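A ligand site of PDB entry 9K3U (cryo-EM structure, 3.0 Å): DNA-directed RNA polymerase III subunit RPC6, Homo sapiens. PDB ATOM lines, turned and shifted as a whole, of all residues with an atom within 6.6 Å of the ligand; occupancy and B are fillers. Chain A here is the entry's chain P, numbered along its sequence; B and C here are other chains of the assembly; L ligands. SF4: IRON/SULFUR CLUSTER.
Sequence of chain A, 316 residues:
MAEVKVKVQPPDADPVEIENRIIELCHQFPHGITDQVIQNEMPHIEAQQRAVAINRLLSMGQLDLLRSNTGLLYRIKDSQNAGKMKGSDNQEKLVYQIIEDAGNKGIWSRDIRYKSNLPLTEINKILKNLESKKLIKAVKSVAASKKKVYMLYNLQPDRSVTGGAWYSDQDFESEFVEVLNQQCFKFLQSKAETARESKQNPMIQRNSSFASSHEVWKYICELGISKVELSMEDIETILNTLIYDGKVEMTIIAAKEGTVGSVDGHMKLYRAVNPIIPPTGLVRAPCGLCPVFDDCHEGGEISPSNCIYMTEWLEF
The side-chain sulfur (SG) of Cys 307 binds an iron atom (FE4) of the ligand (2.5 Å).
A sulfur (S4) of the ligand lies close to the side-chain sulfur (SG) of Cys 290 (3.1 Å).
Merely in contact with the ligand: Cys 287 (3.3 Å), Cys 296 (3.9 Å), Ile 302 (3.8 Å), Pro 304 (3.6 Å), Tyr 309 (3.5 Å), Met 310 (3.4 Å), Phe 38 of chain B (3.5 Å) and Asn 445 of chain C (3.8 Å).
Of the 26 residues printed, 10 come within 4 Å of the ligand.
The guanidinium group (NH1) of Arg 449 of chain C sits at hydrogen-bond distance from the backbone carbonyl oxygen (O) of Pro 304 (3.2 Å).
The side-chain hydroxyl (OG) of Ser 442 of chain C sits close to the side-chain sulfur (SG) of Cys 287.
The backbone carbonyl oxygen (O) of Cys 296 sits at hydrogen-bond distance from the side-chain amino group (NZ) of Lys 441 of chain C, 3.3 Å away.
The side-chain amide oxygen of Asn 445 of chain C is in hydrogen-bond range of the side-chain sulfur of Cys 296.
SG of Cys 307 sits close to N of Met 310, 3.4 Å away.
SG of Cys 307 sits close to N of Tyr 309, at 3.2 Å.
The side-chain sulfur of Cys 290 sits close to the backbone NH of Val 292 (3.7 Å).
SG of Cys 290 lies within hydrogen-bond range of N of Phe 293, 3.7 Å away.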
ATOM      1  N   PRO A 286      33.868  22.019  11.585  1.00  0.00           N
ATOM      2  CA  PRO A 286      32.901  23.117  11.470  1.00  0.00           C
ATOM      3  C   PRO A 286      32.264  23.512  12.797  1.00  0.00           C
ATOM      4  O   PRO A 286      31.794  24.651  12.922  1.00  0.00           O
ATOM      5  CB  PRO A 286      31.855  22.572  10.502  1.00  0.00           C
ATOM      6  CG  PRO A 286      32.555  21.498   9.740  1.00  0.00           C
ATOM      7  CD  PRO A 286      33.529  20.894  10.688  1.00  0.00           C
ATOM      8  N   CYS A 287      32.245  22.620  13.780  1.00  0.00           N
ATOM      9  CA  CYS A 287      31.607  22.934  15.054  1.00  0.00           C
ATOM     10  C   CYS A 287      32.379  23.998  15.816  1.00  0.00           C
ATOM     11  O   CYS A 287      31.770  24.842  16.496  1.00  0.00           O
ATOM     12  CB  CYS A 287      31.473  21.669  15.908  1.00  0.00           C
ATOM     13  SG  CYS A 287      30.644  20.295  15.076  1.00  0.00           S
ATOM     14  N   GLY A 288      33.711  23.998  15.726  1.00  0.00           N
ATOM     15  CA  GLY A 288      34.508  24.968  16.450  1.00  0.00           C
ATOM     16  C   GLY A 288      34.479  26.362  15.871  1.00  0.00           C
ATOM     17  O   GLY A 288      34.737  27.328  16.597  1.00  0.00           O
ATOM     18  N   CYS A 290      31.679  27.620  14.253  1.00  0.00           N
ATOM     19  CA  CYS A 290      30.283  27.938  13.959  1.00  0.00           C
ATOM     20  C   CYS A 290      29.855  29.174  14.754  1.00  0.00           C
ATOM     21  O   CYS A 290      30.074  29.227  15.967  1.00  0.00           O
ATOM     22  CB  CYS A 290      29.397  26.747  14.302  1.00  0.00           C
ATOM     23  SG  CYS A 290      27.647  27.003  13.967  1.00  0.00           S
ATOM     24  N   PRO A 291      29.238  30.174  14.113  1.00  0.00           N
ATOM     25  CA  PRO A 291      28.847  31.378  14.854  1.00  0.00           C
ATOM     26  C   PRO A 291      27.586  31.225  15.672  1.00  0.00           C
ATOM     27  O   PRO A 291      27.387  31.993  16.627  1.00  0.00           O
ATOM     28  CB  PRO A 291      28.662  32.420  13.743  1.00  0.00           C
ATOM     29  CG  PRO A 291      28.225  31.623  12.568  1.00  0.00           C
ATOM     30  CD  PRO A 291      28.920  30.274  12.678  1.00  0.00           C
ATOM     31  N   VAL A 292      26.722  30.260  15.335  1.00  0.00           N
ATOM     32  CA  VAL A 292      25.491  30.024  16.079  1.00  0.00           C
ATOM     33  C   VAL A 292      25.659  28.765  16.916  1.00  0.00           C
ATOM     34  O   VAL A 292      24.700  28.057  17.222  1.00  0.00           O
ATOM     35  CB  VAL A 292      24.276  29.912  15.130  1.00  0.00           C
ATOM     36  CG1 VAL A 292      24.329  28.618  14.329  1.00  0.00           C
ATOM     37  CG2 VAL A 292      22.974  30.036  15.899  1.00  0.00           C
ATOM     38  N   PHE A 293      26.920  28.479  17.280  1.00  0.00           N
ATOM     39  CA  PHE A 293      27.212  27.283  18.068  1.00  0.00           C
ATOM     40  C   PHE A 293      26.430  27.240  19.365  1.00  0.00           C
ATOM     41  O   PHE A 293      26.160  26.159  19.893  1.00  0.00           O
ATOM     42  CB  PHE A 293      28.714  27.217  18.345  1.00  0.00           C
ATOM     43  CG  PHE A 293      29.105  26.185  19.377  1.00  0.00           C
ATOM     44  CD1 PHE A 293      29.300  24.863  19.012  1.00  0.00           C
ATOM     45  CD2 PHE A 293      29.289  26.553  20.701  1.00  0.00           C
ATOM     46  CE1 PHE A 293      29.665  23.924  19.948  1.00  0.00           C
ATOM     47  CE2 PHE A 293      29.643  25.610  21.645  1.00  0.00           C
ATOM     48  CZ  PHE A 293      29.843  24.298  21.267  1.00  0.00           C
ATOM     49  N   ASP A 294      26.054  28.401  19.912  1.00  0.00           N
ATOM     50  CA  ASP A 294      25.342  28.432  21.180  1.00  0.00           C
ATOM     51  C   ASP A 294      23.964  27.791  21.075  1.00  0.00           C
ATOM     52  O   ASP A 294      23.483  27.192  22.039  1.00  0.00           O
ATOM     53  CB  ASP A 294      25.220  29.869  21.683  1.00  0.00           C
ATOM     54  CG  ASP A 294      26.563  30.520  21.917  1.00  0.00           C
ATOM     55  OD1 ASP A 294      27.525  29.796  22.258  1.00  0.00           O
ATOM     56  OD2 ASP A 294      26.667  31.752  21.768  1.00  0.00           O
ATOM     57  N   ASP A 295      23.311  27.909  19.915  1.00  0.00           N
ATOM     58  CA  ASP A 295      21.959  27.393  19.736  1.00  0.00           C
ATOM     59  C   ASP A 295      21.930  25.952  19.253  1.00  0.00           C
ATOM     60  O   ASP A 295      20.874  25.485  18.816  1.00  0.00           O
ATOM     61  CB  ASP A 295      21.202  28.282  18.740  1.00  0.00           C
ATOM     62  CG  ASP A 295      21.296  29.754  19.093  1.00  0.00           C
ATOM     63  OD1 ASP A 295      21.495  30.074  20.281  1.00  0.00           O
ATOM     64  OD2 ASP A 295      21.170  30.587  18.173  1.00  0.00           O
ATOM     65  N   CYS A 296      23.051  25.233  19.319  1.00  0.00           N
ATOM     66  CA  CYS A 296      23.064  23.845  18.880  1.00  0.00           C
ATOM     67  C   CYS A 296      22.236  22.973  19.817  1.00  0.00           C
ATOM     68  O   CYS A 296      22.259  23.142  21.039  1.00  0.00           O
ATOM     69  CB  CYS A 296      24.506  23.323  18.831  1.00  0.00           C
ATOM     70  SG  CYS A 296      24.642  21.557  18.470  1.00  0.00           S
ATOM     71  N   HIS A 297      21.487  22.043  19.222  1.00  0.00           N
ATOM     72  CA  HIS A 297      20.647  21.141  19.996  1.00  0.00           C
ATOM     73  C   HIS A 297      20.398  19.885  19.187  1.00  0.00           C
ATOM     74  O   HIS A 297      20.420  19.903  17.957  1.00  0.00           O
ATOM     75  CB  HIS A 297      19.321  21.801  20.384  1.00  0.00           C
ATOM     76  CG  HIS A 297      18.534  21.025  21.385  1.00  0.00           C
ATOM     77  ND1 HIS A 297      19.070  20.564  22.573  1.00  0.00           N
ATOM     78  CD2 HIS A 297      17.236  20.623  21.393  1.00  0.00           C
ATOM     79  CE1 HIS A 297      18.146  19.915  23.256  1.00  0.00           C
ATOM     80  NE2 HIS A 297      17.020  19.933  22.558  1.00  0.00           N
ATOM     81  N   ILE A 302      18.176  23.752  14.489  1.00  0.00           N
ATOM     82  CA  ILE A 302      19.620  23.685  14.330  1.00  0.00           C
ATOM     83  C   ILE A 302      20.067  22.372  14.958  1.00  0.00           C
ATOM     84  O   ILE A 302      20.275  22.277  16.169  1.00  0.00           O
ATOM     85  CB  ILE A 302      20.321  24.892  14.974  1.00  0.00           C
ATOM     86  CG1 ILE A 302      19.760  26.189  14.385  1.00  0.00           C
ATOM     87  CG2 ILE A 302      21.824  24.813  14.740  1.00  0.00           C
ATOM     88  CD1 ILE A 302      20.342  27.449  14.999  1.00  0.00           C
ATOM     89  N   SER A 303      20.225  21.347  14.124  1.00  0.00           N
ATOM     90  CA  SER A 303      20.622  20.015  14.570  1.00  0.00           C
ATOM     91  C   SER A 303      21.810  19.538  13.745  1.00  0.00           C
ATOM     92  O   SER A 303      21.894  19.834  12.551  1.00  0.00           O
ATOM     93  CB  SER A 303      19.464  19.021  14.429  1.00  0.00           C
ATOM     94  OG  SER A 303      19.837  17.729  14.875  1.00  0.00           O
ATOM     95  N   PRO A 304      22.736  18.798  14.357  1.00  0.00           N
ATOM     96  CA  PRO A 304      23.886  18.297  13.591  1.00  0.00           C
ATOM     97  C   PRO A 304      23.504  17.353  12.463  1.00  0.00           C
ATOM     98  O   PRO A 304      24.269  17.226  11.494  1.00  0.00           O
ATOM     99  CB  PRO A 304      24.737  17.580  14.649  1.00  0.00           C
ATOM    100  CG  PRO A 304      23.788  17.251  15.747  1.00  0.00           C
ATOM    101  CD  PRO A 304      22.789  18.369  15.770  1.00  0.00           C
ATOM    102  N   SER A 305      22.341  16.703  12.546  1.00  0.00           N
ATOM    103  CA  SER A 305      21.936  15.775  11.493  1.00  0.00           C
ATOM    104  C   SER A 305      21.667  16.519  10.186  1.00  0.00           C
ATOM    105  O   SER A 305      22.078  16.061   9.115  1.00  0.00           O
ATOM    106  CB  SER A 305      20.698  14.998  11.936  1.00  0.00           C
ATOM    107  OG  SER A 305      19.632  15.871  12.246  1.00  0.00           O
ATOM    108  N   ASN A 306      20.982  17.654  10.261  1.00  0.00           N
ATOM    109  CA  ASN A 306      20.630  18.443   9.086  1.00  0.00           C
ATOM    110  C   ASN A 306      21.428  19.742   9.022  1.00  0.00           C
ATOM    111  O   ASN A 306      20.912  20.778   8.589  1.00  0.00           O
ATOM    112  CB  ASN A 306      19.131  18.742   9.060  1.00  0.00           C
ATOM    113  CG  ASN A 306      18.655  19.423  10.326  1.00  0.00           C
ATOM    114  OD1 ASN A 306      19.439  19.984  11.086  1.00  0.00           O
ATOM    115  ND2 ASN A 306      17.344  19.389  10.559  1.00  0.00           N
ATOM    116  N   CYS A 307      22.692  19.708   9.442  1.00  0.00           N
ATOM    117  CA  CYS A 307      23.517  20.902   9.433  1.00  0.00           C
ATOM    118  C   CYS A 307      24.012  21.196   8.021  1.00  0.00           C
ATOM    119  O   CYS A 307      24.257  20.293   7.228  1.00  0.00           O
ATOM    120  CB  CYS A 307      24.712  20.734  10.373  1.00  0.00           C
ATOM    121  SG  CYS A 307      25.919  22.074  10.289  1.00  0.00           S
ATOM    122  N   ILE A 308      24.157  22.486   7.724  1.00  0.00           N
ATOM    123  CA  ILE A 308      24.683  22.897   6.422  1.00  0.00           C
ATOM    124  C   ILE A 308      26.202  23.065   6.464  1.00  0.00           C
ATOM    125  O   ILE A 308      26.879  22.771   5.479  1.00  0.00           O
ATOM    126  CB  ILE A 308      23.996  24.198   5.961  1.00  0.00           C
ATOM    127  CG1 ILE A 308      22.476  24.041   5.960  1.00  0.00           C
ATOM    128  CG2 ILE A 308      24.495  24.601   4.572  1.00  0.00           C
ATOM    129  CD1 ILE A 308      21.955  22.915   5.081  1.00  0.00           C
ATOM    130  N   TYR A 309      26.752  23.549   7.581  1.00  0.00           N
ATOM    131  CA  TYR A 309      28.198  23.714   7.696  1.00  0.00           C
ATOM    132  C   TYR A 309      28.901  22.385   7.488  1.00  0.00           C
ATOM    133  O   TYR A 309      29.779  22.261   6.619  1.00  0.00           O
ATOM    134  CB  TYR A 309      28.554  24.304   9.050  1.00  0.00           C
ATOM    135  CG  TYR A 309      27.941  25.665   9.317  1.00  0.00           C
ATOM    136  CD1 TYR A 309      28.548  26.822   8.875  1.00  0.00           C
ATOM    137  CD2 TYR A 309      26.741  25.776  10.019  1.00  0.00           C
ATOM    138  CE1 TYR A 309      27.994  28.066   9.113  1.00  0.00           C
ATOM    139  CE2 TYR A 309      26.177  27.016  10.265  1.00  0.00           C
ATOM    140  CZ  TYR A 309      26.803  28.154   9.814  1.00  0.00           C
ATOM    141  OH  TYR A 309      26.235  29.384  10.050  1.00  0.00           O
ATOM    142  N   MET A 310      28.544  21.370   8.275  1.00  0.00           N
ATOM    143  CA  MET A 310      29.178  20.062   8.146  1.00  0.00           C
ATOM    144  C   MET A 310      28.865  19.427   6.801  1.00  0.00           C
ATOM    145  O   MET A 310      29.708  18.735   6.232  1.00  0.00           O
ATOM    146  CB  MET A 310      28.736  19.147   9.283  1.00  0.00           C
ATOM    147  CG  MET A 310      29.218  19.591  10.655  1.00  0.00           C
ATOM    148  SD  MET A 310      28.859  18.389  11.950  1.00  0.00           S
ATOM    149  CE  MET A 310      27.065  18.453  11.994  1.00  0.00           C
ATOM    150  N   PHE B  38      21.184  29.734   9.301  1.00  0.00           N
ATOM    151  CA  PHE B  38      22.606  29.404   9.272  1.00  0.00           C
ATOM    152  C   PHE B  38      23.339  30.513   8.547  1.00  0.00           C
ATOM    153  O   PHE B  38      23.529  30.457   7.317  1.00  0.00           O
ATOM    154  CB  PHE B  38      22.846  28.048   8.599  1.00  0.00           C
ATOM    155  CG  PHE B  38      22.214  26.892   9.322  1.00  0.00           C
ATOM    156  CD1 PHE B  38      22.891  26.256  10.353  1.00  0.00           C
ATOM    157  CD2 PHE B  38      20.944  26.449   8.984  1.00  0.00           C
ATOM    158  CE1 PHE B  38      22.314  25.191  11.024  1.00  0.00           C
ATOM    159  CE2 PHE B  38      20.371  25.381   9.647  1.00  0.00           C
ATOM    160  CZ  PHE B  38      21.050  24.758  10.674  1.00  0.00           C
ATOM    161  N   LYS C 441      31.430  19.606  23.073  1.00  0.00           N
ATOM    162  CA  LYS C 441      30.177  19.687  22.328  1.00  0.00           C
ATOM    163  C   LYS C 441      30.396  19.466  20.837  1.00  0.00           C
ATOM    164  O   LYS C 441      29.534  18.906  20.159  1.00  0.00           O
ATOM    165  CB  LYS C 441      29.503  21.026  22.577  1.00  0.00           C
ATOM    166  CG  LYS C 441      28.085  21.117  22.022  1.00  0.00           C
ATOM    167  CD  LYS C 441      27.308  22.270  22.627  1.00  0.00           C
ATOM    168  CE  LYS C 441      25.898  22.338  22.071  1.00  0.00           C
ATOM    169  NZ  LYS C 441      25.140  23.490  22.627  1.00  0.00           N
ATOM    170  N   SER C 442      31.554  19.887  20.308  1.00  0.00           N
ATOM    171  CA  SER C 442      31.856  19.659  18.896  1.00  0.00           C
ATOM    172  C   SER C 442      31.996  18.171  18.607  1.00  0.00           C
ATOM    173  O   SER C 442      31.460  17.676  17.611  1.00  0.00           O
ATOM    174  CB  SER C 442      33.129  20.409  18.522  1.00  0.00           C
ATOM    175  OG  SER C 442      33.585  20.025  17.231  1.00  0.00           O
ATOM    176  N   ASN C 445      28.577  16.629  18.655  1.00  0.00           N
ATOM    177  CA  ASN C 445      27.830  16.893  17.435  1.00  0.00           C
ATOM    178  C   ASN C 445      28.355  16.066  16.268  1.00  0.00           C
ATOM    179  O   ASN C 445      27.572  15.582  15.440  1.00  0.00           O
ATOM    180  CB  ASN C 445      27.888  18.378  17.097  1.00  0.00           C
ATOM    181  CG  ASN C 445      27.273  19.248  18.181  1.00  0.00           C
ATOM    182  OD1 ASN C 445      26.352  18.826  18.882  1.00  0.00           O
ATOM    183  ND2 ASN C 445      27.777  20.474  18.315  1.00  0.00           N
ATOM    184  N   LEU C 446      29.672  15.878  16.187  1.00  0.00           N
ATOM    185  CA  LEU C 446      30.240  15.055  15.125  1.00  0.00           C
ATOM    186  C   LEU C 446      29.798  13.597  15.258  1.00  0.00           C
ATOM    187  O   LEU C 446      29.445  12.955  14.269  1.00  0.00           O
ATOM    188  CB  LEU C 446      31.765  15.148  15.138  1.00  0.00           C
ATOM    189  CG  LEU C 446      32.364  16.509  14.762  1.00  0.00           C
ATOM    190  CD1 LEU C 446      33.873  16.499  14.980  1.00  0.00           C
ATOM    191  CD2 LEU C 446      32.029  16.884  13.333  1.00  0.00           C
ATOM    192  N   ARG C 449      26.229  13.381  14.164  1.00  0.00           N
ATOM    193  CA  ARG C 449      26.102  13.429  12.708  1.00  0.00           C
ATOM    194  C   ARG C 449      26.506  12.101  12.079  1.00  0.00           C
ATOM    195  O   ARG C 449      25.840  11.636  11.145  1.00  0.00           O
ATOM    196  CB  ARG C 449      26.961  14.567  12.147  1.00  0.00           C
ATOM    197  CG  ARG C 449      27.003  14.647  10.624  1.00  0.00           C
ATOM    198  CD  ARG C 449      25.605  14.707  10.019  1.00  0.00           C
ATOM    199  NE  ARG C 449      25.643  14.914   8.578  1.00  0.00           N
ATOM    200  CZ  ARG C 449      25.724  16.110   7.983  1.00  0.00           C
ATOM    201  NH1 ARG C 449      25.775  17.218   8.704  1.00  0.00           N
ATOM    202  NH2 ARG C 449      25.756  16.182   6.661  1.00  0.00           N
HETATM  203 FE1  SF4 L   1      27.039  24.176  13.124  1.00  0.00          FE
HETATM  204 FE2  SF4 L   1      25.345  23.079  14.979  1.00  0.00          FE
HETATM  205 FE3  SF4 L   1      27.909  22.147  14.740  1.00  0.00          FE
HETATM  206 FE4  SF4 L   1      26.083  21.635  12.769  1.00  0.00          FE
HETATM  207  S1  SF4 L   1      26.015  20.904  14.926  1.00  0.00           S
HETATM  208  S2  SF4 L   1      28.235  22.345  12.497  1.00  0.00           S
HETATM  209  S3  SF4 L   1      24.860  23.563  12.794  1.00  0.00           S
HETATM  210  S4  SF4 L   1      27.267  24.239  15.391  1.00  0.00           S
